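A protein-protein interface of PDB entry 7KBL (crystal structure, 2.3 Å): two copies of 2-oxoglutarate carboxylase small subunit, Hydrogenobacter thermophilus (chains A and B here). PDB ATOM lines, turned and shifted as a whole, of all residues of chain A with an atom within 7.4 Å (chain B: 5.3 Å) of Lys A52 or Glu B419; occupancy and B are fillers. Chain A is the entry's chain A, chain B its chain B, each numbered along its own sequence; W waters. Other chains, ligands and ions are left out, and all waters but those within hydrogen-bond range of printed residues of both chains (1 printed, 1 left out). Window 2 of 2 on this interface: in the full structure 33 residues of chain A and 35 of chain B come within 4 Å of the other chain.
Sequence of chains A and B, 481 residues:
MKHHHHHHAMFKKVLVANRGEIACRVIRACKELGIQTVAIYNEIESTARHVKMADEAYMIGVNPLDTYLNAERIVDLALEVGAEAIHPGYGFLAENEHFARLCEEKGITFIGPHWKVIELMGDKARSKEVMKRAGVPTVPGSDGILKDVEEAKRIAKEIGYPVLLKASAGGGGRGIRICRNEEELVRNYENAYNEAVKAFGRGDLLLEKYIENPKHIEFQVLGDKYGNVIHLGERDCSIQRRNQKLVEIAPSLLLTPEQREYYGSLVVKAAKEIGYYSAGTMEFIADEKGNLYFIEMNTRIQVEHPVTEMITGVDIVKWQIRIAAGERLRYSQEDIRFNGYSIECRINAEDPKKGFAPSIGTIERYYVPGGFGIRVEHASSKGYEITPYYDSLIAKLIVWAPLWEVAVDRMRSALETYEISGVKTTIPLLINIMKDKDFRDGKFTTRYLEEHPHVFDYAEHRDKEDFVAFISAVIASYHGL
Of the 17 printed residues of chain A, 4 touch a printed residue of chain B. Printed residues of chain A that touch a printed residue of chain B: Arg A49, Lys A52, Met A53 and Ser A381. Hydrophobic or aromatic side chains of chain A within 4 Å of the printed part of chain B: Met A53. Of the 8 printed residues of chain B, 4 touch a printed residue of chain A.
Among the printed residues, merely in contact across the chains: Arg A49 with Tyr B367 (3.3 Å), Met A53 with Thr B417 (3.9 Å) and Ser A381 with Tyr B367 (3.4 Å).
Of the printed residues of chain B, Arg A49 touches Tyr B367 and Glu B419. Of chain B, only Glu B419 comes within 4 Å of Lys A52. Of the printed residues of chain B, Met A53 touches Thr B417. Of the printed residues of chain A, Tyr B366 touches Ser A381. Of the printed residues of chain A, Tyr B367 touches Arg A49 and Ser A381. Of the printed residues of chain A, Thr B417 touches Met A53 (3.9 Å). Ile B420 touches none of the printed residues of chain A. The nearest printed residue of chain B that does not touch Met A53 is Tyr B367 (4.5 Å).
No position is printed for both chains. Of the 6 pairs that touch across the chains among the printed residues, none has its exchanged pair printed and touching as well.
The guanidinium group (NH2) of Arg A49 lies within salt-bridge range of the side-chain carboxylate (OE1) of Glu B419, 2.5 Å away. OE1 of Glu B419 is in salt-bridge range of NZ of Lys A52, at 3.2 Å. The side-chain hydroxyl (OG) of Ser A381 sits at hydrogen-bond distance from the backbone carbonyl oxygen (O) of Tyr B366, 3.3 Å away.
Water W1 bridges the side-chain hydroxyl of Ser A381 (2.9 Å) and the backbone NH of Tyr B366 (3.1 Å).
The side-chain carboxylate (OE2) of Glu B419 lies within salt-bridge range of the guanidinium group (NE) of Arg B365, at 3.1 Å. OH of Tyr B366 is in hydrogen-bond range of OH of Tyr B418. O of Glu B419 lies within hydrogen-bond range of N of Tyr B367 (3.1 Å).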
ATOM      1  N   ILE A  27     -29.172   8.223  10.569  1.00  0.00           N
ATOM      2  CA  ILE A  27     -29.316   6.866  11.042  1.00  0.00           C
ATOM      3  C   ILE A  27     -30.614   6.717  11.822  1.00  0.00           C
ATOM      4  O   ILE A  27     -31.299   5.700  11.705  1.00  0.00           O
ATOM      5  CB  ILE A  27     -28.081   6.461  11.866  1.00  0.00           C
ATOM      6  CG1 ILE A  27     -26.898   6.223  10.931  1.00  0.00           C
ATOM      7  CG2 ILE A  27     -28.395   5.226  12.781  1.00  0.00           C
ATOM      8  CD1 ILE A  27     -25.616   6.243  11.675  1.00  0.00           C
ATOM      9  N   LYS A  31     -33.587   4.093  11.043  1.00  0.00           N
ATOM     10  CA  LYS A  31     -34.079   3.090  11.993  1.00  0.00           C
ATOM     11  C   LYS A  31     -35.577   3.202  12.160  1.00  0.00           C
ATOM     12  O   LYS A  31     -36.285   2.198  12.123  1.00  0.00           O
ATOM     13  CB  LYS A  31     -33.400   3.228  13.353  1.00  0.00           C
ATOM     14  CG  LYS A  31     -31.932   2.843  13.383  1.00  0.00           C
ATOM     15  CD  LYS A  31     -31.318   3.103  14.730  1.00  0.00           C
ATOM     16  CE  LYS A  31     -31.781   2.121  15.767  1.00  0.00           C
ATOM     17  NZ  LYS A  31     -31.265   0.706  15.563  1.00  0.00           N
ATOM     18  N   ALA A  39     -22.336   2.666   8.214  1.00  0.00           N
ATOM     19  CA  ALA A  39     -21.500   3.808   8.540  1.00  0.00           C
ATOM     20  C   ALA A  39     -20.130   3.636   7.911  1.00  0.00           C
ATOM     21  O   ALA A  39     -19.692   2.520   7.629  1.00  0.00           O
ATOM     22  CB  ALA A  39     -21.345   3.987  10.045  1.00  0.00           C
ATOM     23  N   GLU A  45     -11.466   7.414  14.655  1.00  0.00           N
ATOM     24  CA  GLU A  45     -12.851   7.486  15.112  1.00  0.00           C
ATOM     25  C   GLU A  45     -13.426   6.106  15.344  1.00  0.00           C
ATOM     26  O   GLU A  45     -14.589   5.837  15.029  1.00  0.00           O
ATOM     27  CB  GLU A  45     -13.703   8.211  14.068  1.00  0.00           C
ATOM     28  CG  GLU A  45     -13.750   9.687  14.197  1.00  0.00           C
ATOM     29  CD  GLU A  45     -14.760  10.299  13.231  1.00  0.00           C
ATOM     30  OE1 GLU A  45     -14.735   9.958  11.994  1.00  0.00           O
ATOM     31  OE2 GLU A  45     -15.579  11.105  13.731  1.00  0.00           O
ATOM     32  N   SER A  46     -12.639   5.193  15.886  1.00  0.00           N
ATOM     33  CA  SER A  46     -13.143   3.829  16.019  1.00  0.00           C
ATOM     34  C   SER A  46     -14.370   3.775  16.932  1.00  0.00           C
ATOM     35  O   SER A  46     -15.277   2.964  16.710  1.00  0.00           O
ATOM     36  CB  SER A  46     -12.025   2.946  16.571  1.00  0.00           C
ATOM     37  OG  SER A  46     -11.500   3.562  17.737  1.00  0.00           O
ATOM     38  N   THR A  47     -14.458   4.702  17.884  1.00  0.00           N
ATOM     39  CA  THR A  47     -15.499   4.741  18.897  1.00  0.00           C
ATOM     40  C   THR A  47     -16.621   5.739  18.588  1.00  0.00           C
ATOM     41  O   THR A  47     -17.438   6.032  19.464  1.00  0.00           O
ATOM     42  CB  THR A  47     -14.859   5.107  20.234  1.00  0.00           C
ATOM     43  OG1 THR A  47     -14.381   6.464  20.185  1.00  0.00           O
ATOM     44  CG2 THR A  47     -13.668   4.187  20.524  1.00  0.00           C
ATOM     45  N   ALA A  48     -16.653   6.301  17.390  1.00  0.00           N
ATOM     46  CA  ALA A  48     -17.607   7.354  17.096  1.00  0.00           C
ATOM     47  C   ALA A  48     -19.044   6.876  17.316  1.00  0.00           C
ATOM     48  O   ALA A  48     -19.381   5.706  17.125  1.00  0.00           O
ATOM     49  CB  ALA A  48     -17.416   7.847  15.660  1.00  0.00           C
ATOM     50  N   ARG A  49     -19.895   7.810  17.734  1.00  0.00           N
ATOM     51  CA  ARG A  49     -21.293   7.488  17.992  1.00  0.00           C
ATOM     52  C   ARG A  49     -21.965   6.899  16.752  1.00  0.00           C
ATOM     53  O   ARG A  49     -22.707   5.912  16.840  1.00  0.00           O
ATOM     54  CB  ARG A  49     -22.047   8.746  18.417  1.00  0.00           C
ATOM     55  CG  ARG A  49     -23.330   8.453  19.180  1.00  0.00           C
ATOM     56  CD  ARG A  49     -22.836   7.964  20.519  1.00  0.00           C
ATOM     57  NE  ARG A  49     -23.290   6.676  20.847  1.00  0.00           N
ATOM     58  CZ  ARG A  49     -22.813   5.977  21.856  1.00  0.00           C
ATOM     59  NH1 ARG A  49     -21.840   6.436  22.613  1.00  0.00           N
ATOM     60  NH2 ARG A  49     -23.327   4.796  22.070  1.00  0.00           N
ATOM     61  N   HIS A  50     -21.736   7.508  15.578  1.00  0.00           N
ATOM     62  CA  HIS A  50     -22.472   7.048  14.398  1.00  0.00           C
ATOM     63  C   HIS A  50     -22.033   5.661  13.997  1.00  0.00           C
ATOM     64  O   HIS A  50     -22.829   4.911  13.436  1.00  0.00           O
ATOM     65  CB  HIS A  50     -22.312   8.020  13.212  1.00  0.00           C
ATOM     66  CG  HIS A  50     -20.946   8.036  12.596  1.00  0.00           C
ATOM     67  ND1 HIS A  50     -19.907   8.794  13.098  1.00  0.00           N
ATOM     68  CD2 HIS A  50     -20.442   7.382  11.526  1.00  0.00           C
ATOM     69  CE1 HIS A  50     -18.828   8.611  12.363  1.00  0.00           C
ATOM     70  NE2 HIS A  50     -19.126   7.764  11.395  1.00  0.00           N
ATOM     71  N   VAL A  51     -20.801   5.282  14.337  1.00  0.00           N
ATOM     72  CA  VAL A  51     -20.379   3.897  14.131  1.00  0.00           C
ATOM     73  C   VAL A  51     -21.191   2.965  15.011  1.00  0.00           C
ATOM     74  O   VAL A  51     -21.610   1.895  14.580  1.00  0.00           O
ATOM     75  CB  VAL A  51     -18.885   3.723  14.440  1.00  0.00           C
ATOM     76  CG1 VAL A  51     -18.528   2.211  14.434  1.00  0.00           C
ATOM     77  CG2 VAL A  51     -18.066   4.490  13.462  1.00  0.00           C
ATOM     78  N   LYS A  52     -21.319   3.315  16.290  1.00  0.00           N
ATOM     79  CA  LYS A  52     -22.074   2.485  17.209  1.00  0.00           C
ATOM     80  C   LYS A  52     -23.551   2.408  16.843  1.00  0.00           C
ATOM     81  O   LYS A  52     -24.159   1.350  16.994  1.00  0.00           O
ATOM     82  CB  LYS A  52     -21.876   2.980  18.640  1.00  0.00           C
ATOM     83  CG  LYS A  52     -20.505   2.603  19.218  1.00  0.00           C
ATOM     84  CD  LYS A  52     -20.151   3.497  20.385  1.00  0.00           C
ATOM     85  CE  LYS A  52     -19.054   2.913  21.247  1.00  0.00           C
ATOM     86  NZ  LYS A  52     -19.223   3.335  22.690  1.00  0.00           N
ATOM     87  N   MET A  53     -24.150   3.497  16.338  1.00  0.00           N
ATOM     88  CA  MET A  53     -25.590   3.466  16.085  1.00  0.00           C
ATOM     89  C   MET A  53     -25.953   2.672  14.840  1.00  0.00           C
ATOM     90  O   MET A  53     -27.088   2.173  14.738  1.00  0.00           O
ATOM     91  CB  MET A  53     -26.178   4.884  15.937  1.00  0.00           C
ATOM     92  CG  MET A  53     -26.150   5.675  17.196  1.00  0.00           C
ATOM     93  SD  MET A  53     -26.903   7.298  16.996  1.00  0.00           S
ATOM     94  CE  MET A  53     -28.203   6.963  15.879  1.00  0.00           C
ATOM     95  N   ALA A  54     -25.028   2.551  13.896  1.00  0.00           N
ATOM     96  CA  ALA A  54     -25.345   1.934  12.618  1.00  0.00           C
ATOM     97  C   ALA A  54     -25.334   0.428  12.755  1.00  0.00           C
ATOM     98  O   ALA A  54     -24.741  -0.119  13.678  1.00  0.00           O
ATOM     99  CB  ALA A  54     -24.357   2.377  11.535  1.00  0.00           C
ATOM    100  N   ASP A  55     -26.028  -0.245  11.837  1.00  0.00           N
ATOM    101  CA  ASP A  55     -26.054  -1.710  11.871  1.00  0.00           C
ATOM    102  C   ASP A  55     -24.743  -2.313  11.404  1.00  0.00           C
ATOM    103  O   ASP A  55     -24.448  -3.454  11.762  1.00  0.00           O
ATOM    104  CB  ASP A  55     -27.191  -2.291  11.005  1.00  0.00           C
ATOM    105  CG  ASP A  55     -28.567  -1.786  11.400  1.00  0.00           C
ATOM    106  OD1 ASP A  55     -28.940  -1.902  12.608  1.00  0.00           O
ATOM    107  OD2 ASP A  55     -29.261  -1.241  10.492  1.00  0.00           O
ATOM    108  N   GLU A  56     -23.966  -1.562  10.625  1.00  0.00           N
ATOM    109  CA  GLU A  56     -22.812  -2.038   9.871  1.00  0.00           C
ATOM    110  C   GLU A  56     -21.849  -0.867   9.750  1.00  0.00           C
ATOM    111  O   GLU A  56     -22.291   0.255   9.503  1.00  0.00           O
ATOM    112  CB  GLU A  56     -23.255  -2.485   8.470  1.00  0.00           C
ATOM    113  CG  GLU A  56     -22.798  -3.836   7.941  1.00  0.00           C
ATOM    114  CD  GLU A  56     -23.315  -4.077   6.492  1.00  0.00           C
ATOM    115  OE1 GLU A  56     -22.565  -4.628   5.662  1.00  0.00           O
ATOM    116  OE2 GLU A  56     -24.473  -3.711   6.172  1.00  0.00           O
ATOM    117  N   ALA A  57     -20.554  -1.102   9.932  1.00  0.00           N
ATOM    118  CA  ALA A  57     -19.611  -0.008   9.776  1.00  0.00           C
ATOM    119  C   ALA A  57     -18.259  -0.476   9.242  1.00  0.00           C
ATOM    120  O   ALA A  57     -17.770  -1.554   9.597  1.00  0.00           O
ATOM    121  CB  ALA A  57     -19.423   0.737  11.084  1.00  0.00           C
ATOM    122  N   SER A 381     -20.250  11.859  24.082  1.00  0.00           N
ATOM    123  CA  SER A 381     -20.262  11.357  25.470  1.00  0.00           C
ATOM    124  C   SER A 381     -18.945  11.786  26.115  1.00  0.00           C
ATOM    125  O   SER A 381     -18.092  12.391  25.458  1.00  0.00           O
ATOM    126  CB  SER A 381     -20.336   9.827  25.556  1.00  0.00           C
ATOM    127  OG  SER A 381     -21.495   9.280  24.964  1.00  0.00           O
ATOM    128  N   ARG B 365     -20.301   4.109  30.631  1.00  0.00           N
ATOM    129  CA  ARG B 365     -20.739   4.661  29.354  1.00  0.00           C
ATOM    130  C   ARG B 365     -22.166   5.196  29.460  1.00  0.00           C
ATOM    131  O   ARG B 365     -23.021   4.622  30.157  1.00  0.00           O
ATOM    132  CB  ARG B 365     -20.626   3.611  28.244  1.00  0.00           C
ATOM    133  CG  ARG B 365     -19.166   3.306  27.888  1.00  0.00           C
ATOM    134  CD  ARG B 365     -18.928   2.456  26.636  1.00  0.00           C
ATOM    135  NE  ARG B 365     -19.491   1.104  26.698  1.00  0.00           N
ATOM    136  CZ  ARG B 365     -18.984   0.076  27.392  1.00  0.00           C
ATOM    137  NH1 ARG B 365     -17.895   0.219  28.147  1.00  0.00           N
ATOM    138  NH2 ARG B 365     -19.591  -1.111  27.348  1.00  0.00           N
ATOM    139  N   TYR B 366     -22.405   6.334  28.786  1.00  0.00           N
ATOM    140  CA  TYR B 366     -23.640   7.087  28.963  1.00  0.00           C
ATOM    141  C   TYR B 366     -23.822   8.053  27.785  1.00  0.00           C
ATOM    142  O   TYR B 366     -23.246   9.145  27.778  1.00  0.00           O
ATOM    143  CB  TYR B 366     -23.647   7.831  30.288  1.00  0.00           C
ATOM    144  CG  TYR B 366     -25.042   8.280  30.642  1.00  0.00           C
ATOM    145  CD1 TYR B 366     -26.015   7.343  30.979  1.00  0.00           C
ATOM    146  CD2 TYR B 366     -25.405   9.609  30.592  1.00  0.00           C
ATOM    147  CE1 TYR B 366     -27.271   7.721  31.277  1.00  0.00           C
ATOM    148  CE2 TYR B 366     -26.665  10.006  30.892  1.00  0.00           C
ATOM    149  CZ  TYR B 366     -27.606   9.052  31.234  1.00  0.00           C
ATOM    150  OH  TYR B 366     -28.893   9.396  31.511  1.00  0.00           O
ATOM    151  N   TYR B 367     -24.646   7.650  26.829  1.00  0.00           N
ATOM    152  CA  TYR B 367     -24.994   8.460  25.673  1.00  0.00           C
ATOM    153  C   TYR B 367     -26.494   8.645  25.640  1.00  0.00           C
ATOM    154  O   TYR B 367     -27.228   7.665  25.493  1.00  0.00           O
ATOM    155  CB  TYR B 367     -24.524   7.811  24.369  1.00  0.00           C
ATOM    156  CG  TYR B 367     -25.081   8.558  23.157  1.00  0.00           C
ATOM    157  CD1 TYR B 367     -24.539   9.764  22.749  1.00  0.00           C
ATOM    158  CD2 TYR B 367     -26.193   8.089  22.500  1.00  0.00           C
ATOM    159  CE1 TYR B 367     -25.046  10.448  21.689  1.00  0.00           C
ATOM    160  CE2 TYR B 367     -26.726   8.766  21.431  1.00  0.00           C
ATOM    161  CZ  TYR B 367     -26.153   9.945  21.035  1.00  0.00           C
ATOM    162  OH  TYR B 367     -26.711  10.607  19.981  1.00  0.00           O
ATOM    163  N   THR B 417     -30.453   3.123  20.912  1.00  0.00           N
ATOM    164  CA  THR B 417     -29.303   4.020  20.880  1.00  0.00           C
ATOM    165  C   THR B 417     -28.950   4.567  22.250  1.00  0.00           C
ATOM    166  O   THR B 417     -27.957   5.280  22.377  1.00  0.00           O
ATOM    167  CB  THR B 417     -29.545   5.186  19.897  1.00  0.00           C
ATOM    168  OG1 THR B 417     -30.583   6.055  20.354  1.00  0.00           O
ATOM    169  CG2 THR B 417     -29.934   4.644  18.552  1.00  0.00           C
ATOM    170  N   TYR B 418     -29.725   4.245  23.282  1.00  0.00           N
ATOM    171  CA  TYR B 418     -29.450   4.719  24.633  1.00  0.00           C
ATOM    172  C   TYR B 418     -28.418   3.780  25.283  1.00  0.00           C
ATOM    173  O   TYR B 418     -28.727   2.652  25.645  1.00  0.00           O
ATOM    174  CB  TYR B 418     -30.770   4.810  25.391  1.00  0.00           C
ATOM    175  CG  TYR B 418     -30.813   5.855  26.491  1.00  0.00           C
ATOM    176  CD1 TYR B 418     -29.683   6.178  27.223  1.00  0.00           C
ATOM    177  CD2 TYR B 418     -31.993   6.508  26.794  1.00  0.00           C
ATOM    178  CE1 TYR B 418     -29.731   7.142  28.216  1.00  0.00           C
ATOM    179  CE2 TYR B 418     -32.056   7.470  27.800  1.00  0.00           C
ATOM    180  CZ  TYR B 418     -30.922   7.771  28.505  1.00  0.00           C
ATOM    181  OH  TYR B 418     -30.984   8.736  29.467  1.00  0.00           O
ATOM    182  N   GLU B 419     -27.165   4.225  25.372  1.00  0.00           N
ATOM    183  CA  GLU B 419     -26.065   3.411  25.861  1.00  0.00           C
ATOM    184  C   GLU B 419     -25.860   3.731  27.333  1.00  0.00           C
ATOM    185  O   GLU B 419     -25.642   4.896  27.690  1.00  0.00           O
ATOM    186  CB  GLU B 419     -24.767   3.642  25.074  1.00  0.00           C
ATOM    187  CG  GLU B 419     -23.568   2.735  25.509  1.00  0.00           C
ATOM    188  CD  GLU B 419     -22.273   2.900  24.632  1.00  0.00           C
ATOM    189  OE1 GLU B 419     -22.004   3.994  24.076  1.00  0.00           O
ATOM    190  OE2 GLU B 419     -21.542   1.895  24.469  1.00  0.00           O
ATOM    191  N   ILE B 420     -25.992   2.704  28.180  1.00  0.00           N
ATOM    192  CA  ILE B 420     -25.687   2.764  29.614  1.00  0.00           C
ATOM    193  C   ILE B 420     -24.895   1.504  29.980  1.00  0.00           C
ATOM    194  O   ILE B 420     -25.362   0.385  29.745  1.00  0.00           O
ATOM    195  CB  ILE B 420     -26.947   2.865  30.510  1.00  0.00           C
ATOM    196  CG1 ILE B 420     -27.854   4.020  30.084  1.00  0.00           C
ATOM    197  CG2 ILE B 420     -26.544   3.071  31.977  1.00  0.00           C
ATOM    198  CD1 ILE B 420     -29.168   4.143  30.829  1.00  0.00           C
ATOM    199  N   SER B 421     -23.706   1.681  30.550  1.00  0.00           N
ATOM    200  CA  SER B 421     -22.930   0.593  31.140  1.00  0.00           C
ATOM    201  C   SER B 421     -22.548   0.973  32.570  1.00  0.00           C
ATOM    202  O   SER B 421     -22.663   2.132  32.985  1.00  0.00           O
ATOM    203  CB  SER B 421     -21.681   0.294  30.330  1.00  0.00           C
ATOM    204  OG  SER B 421     -20.705   1.268  30.648  1.00  0.00           O
HETATM  205  O   HOH W   1     -20.619   6.804  26.253  1.00  0.00           O
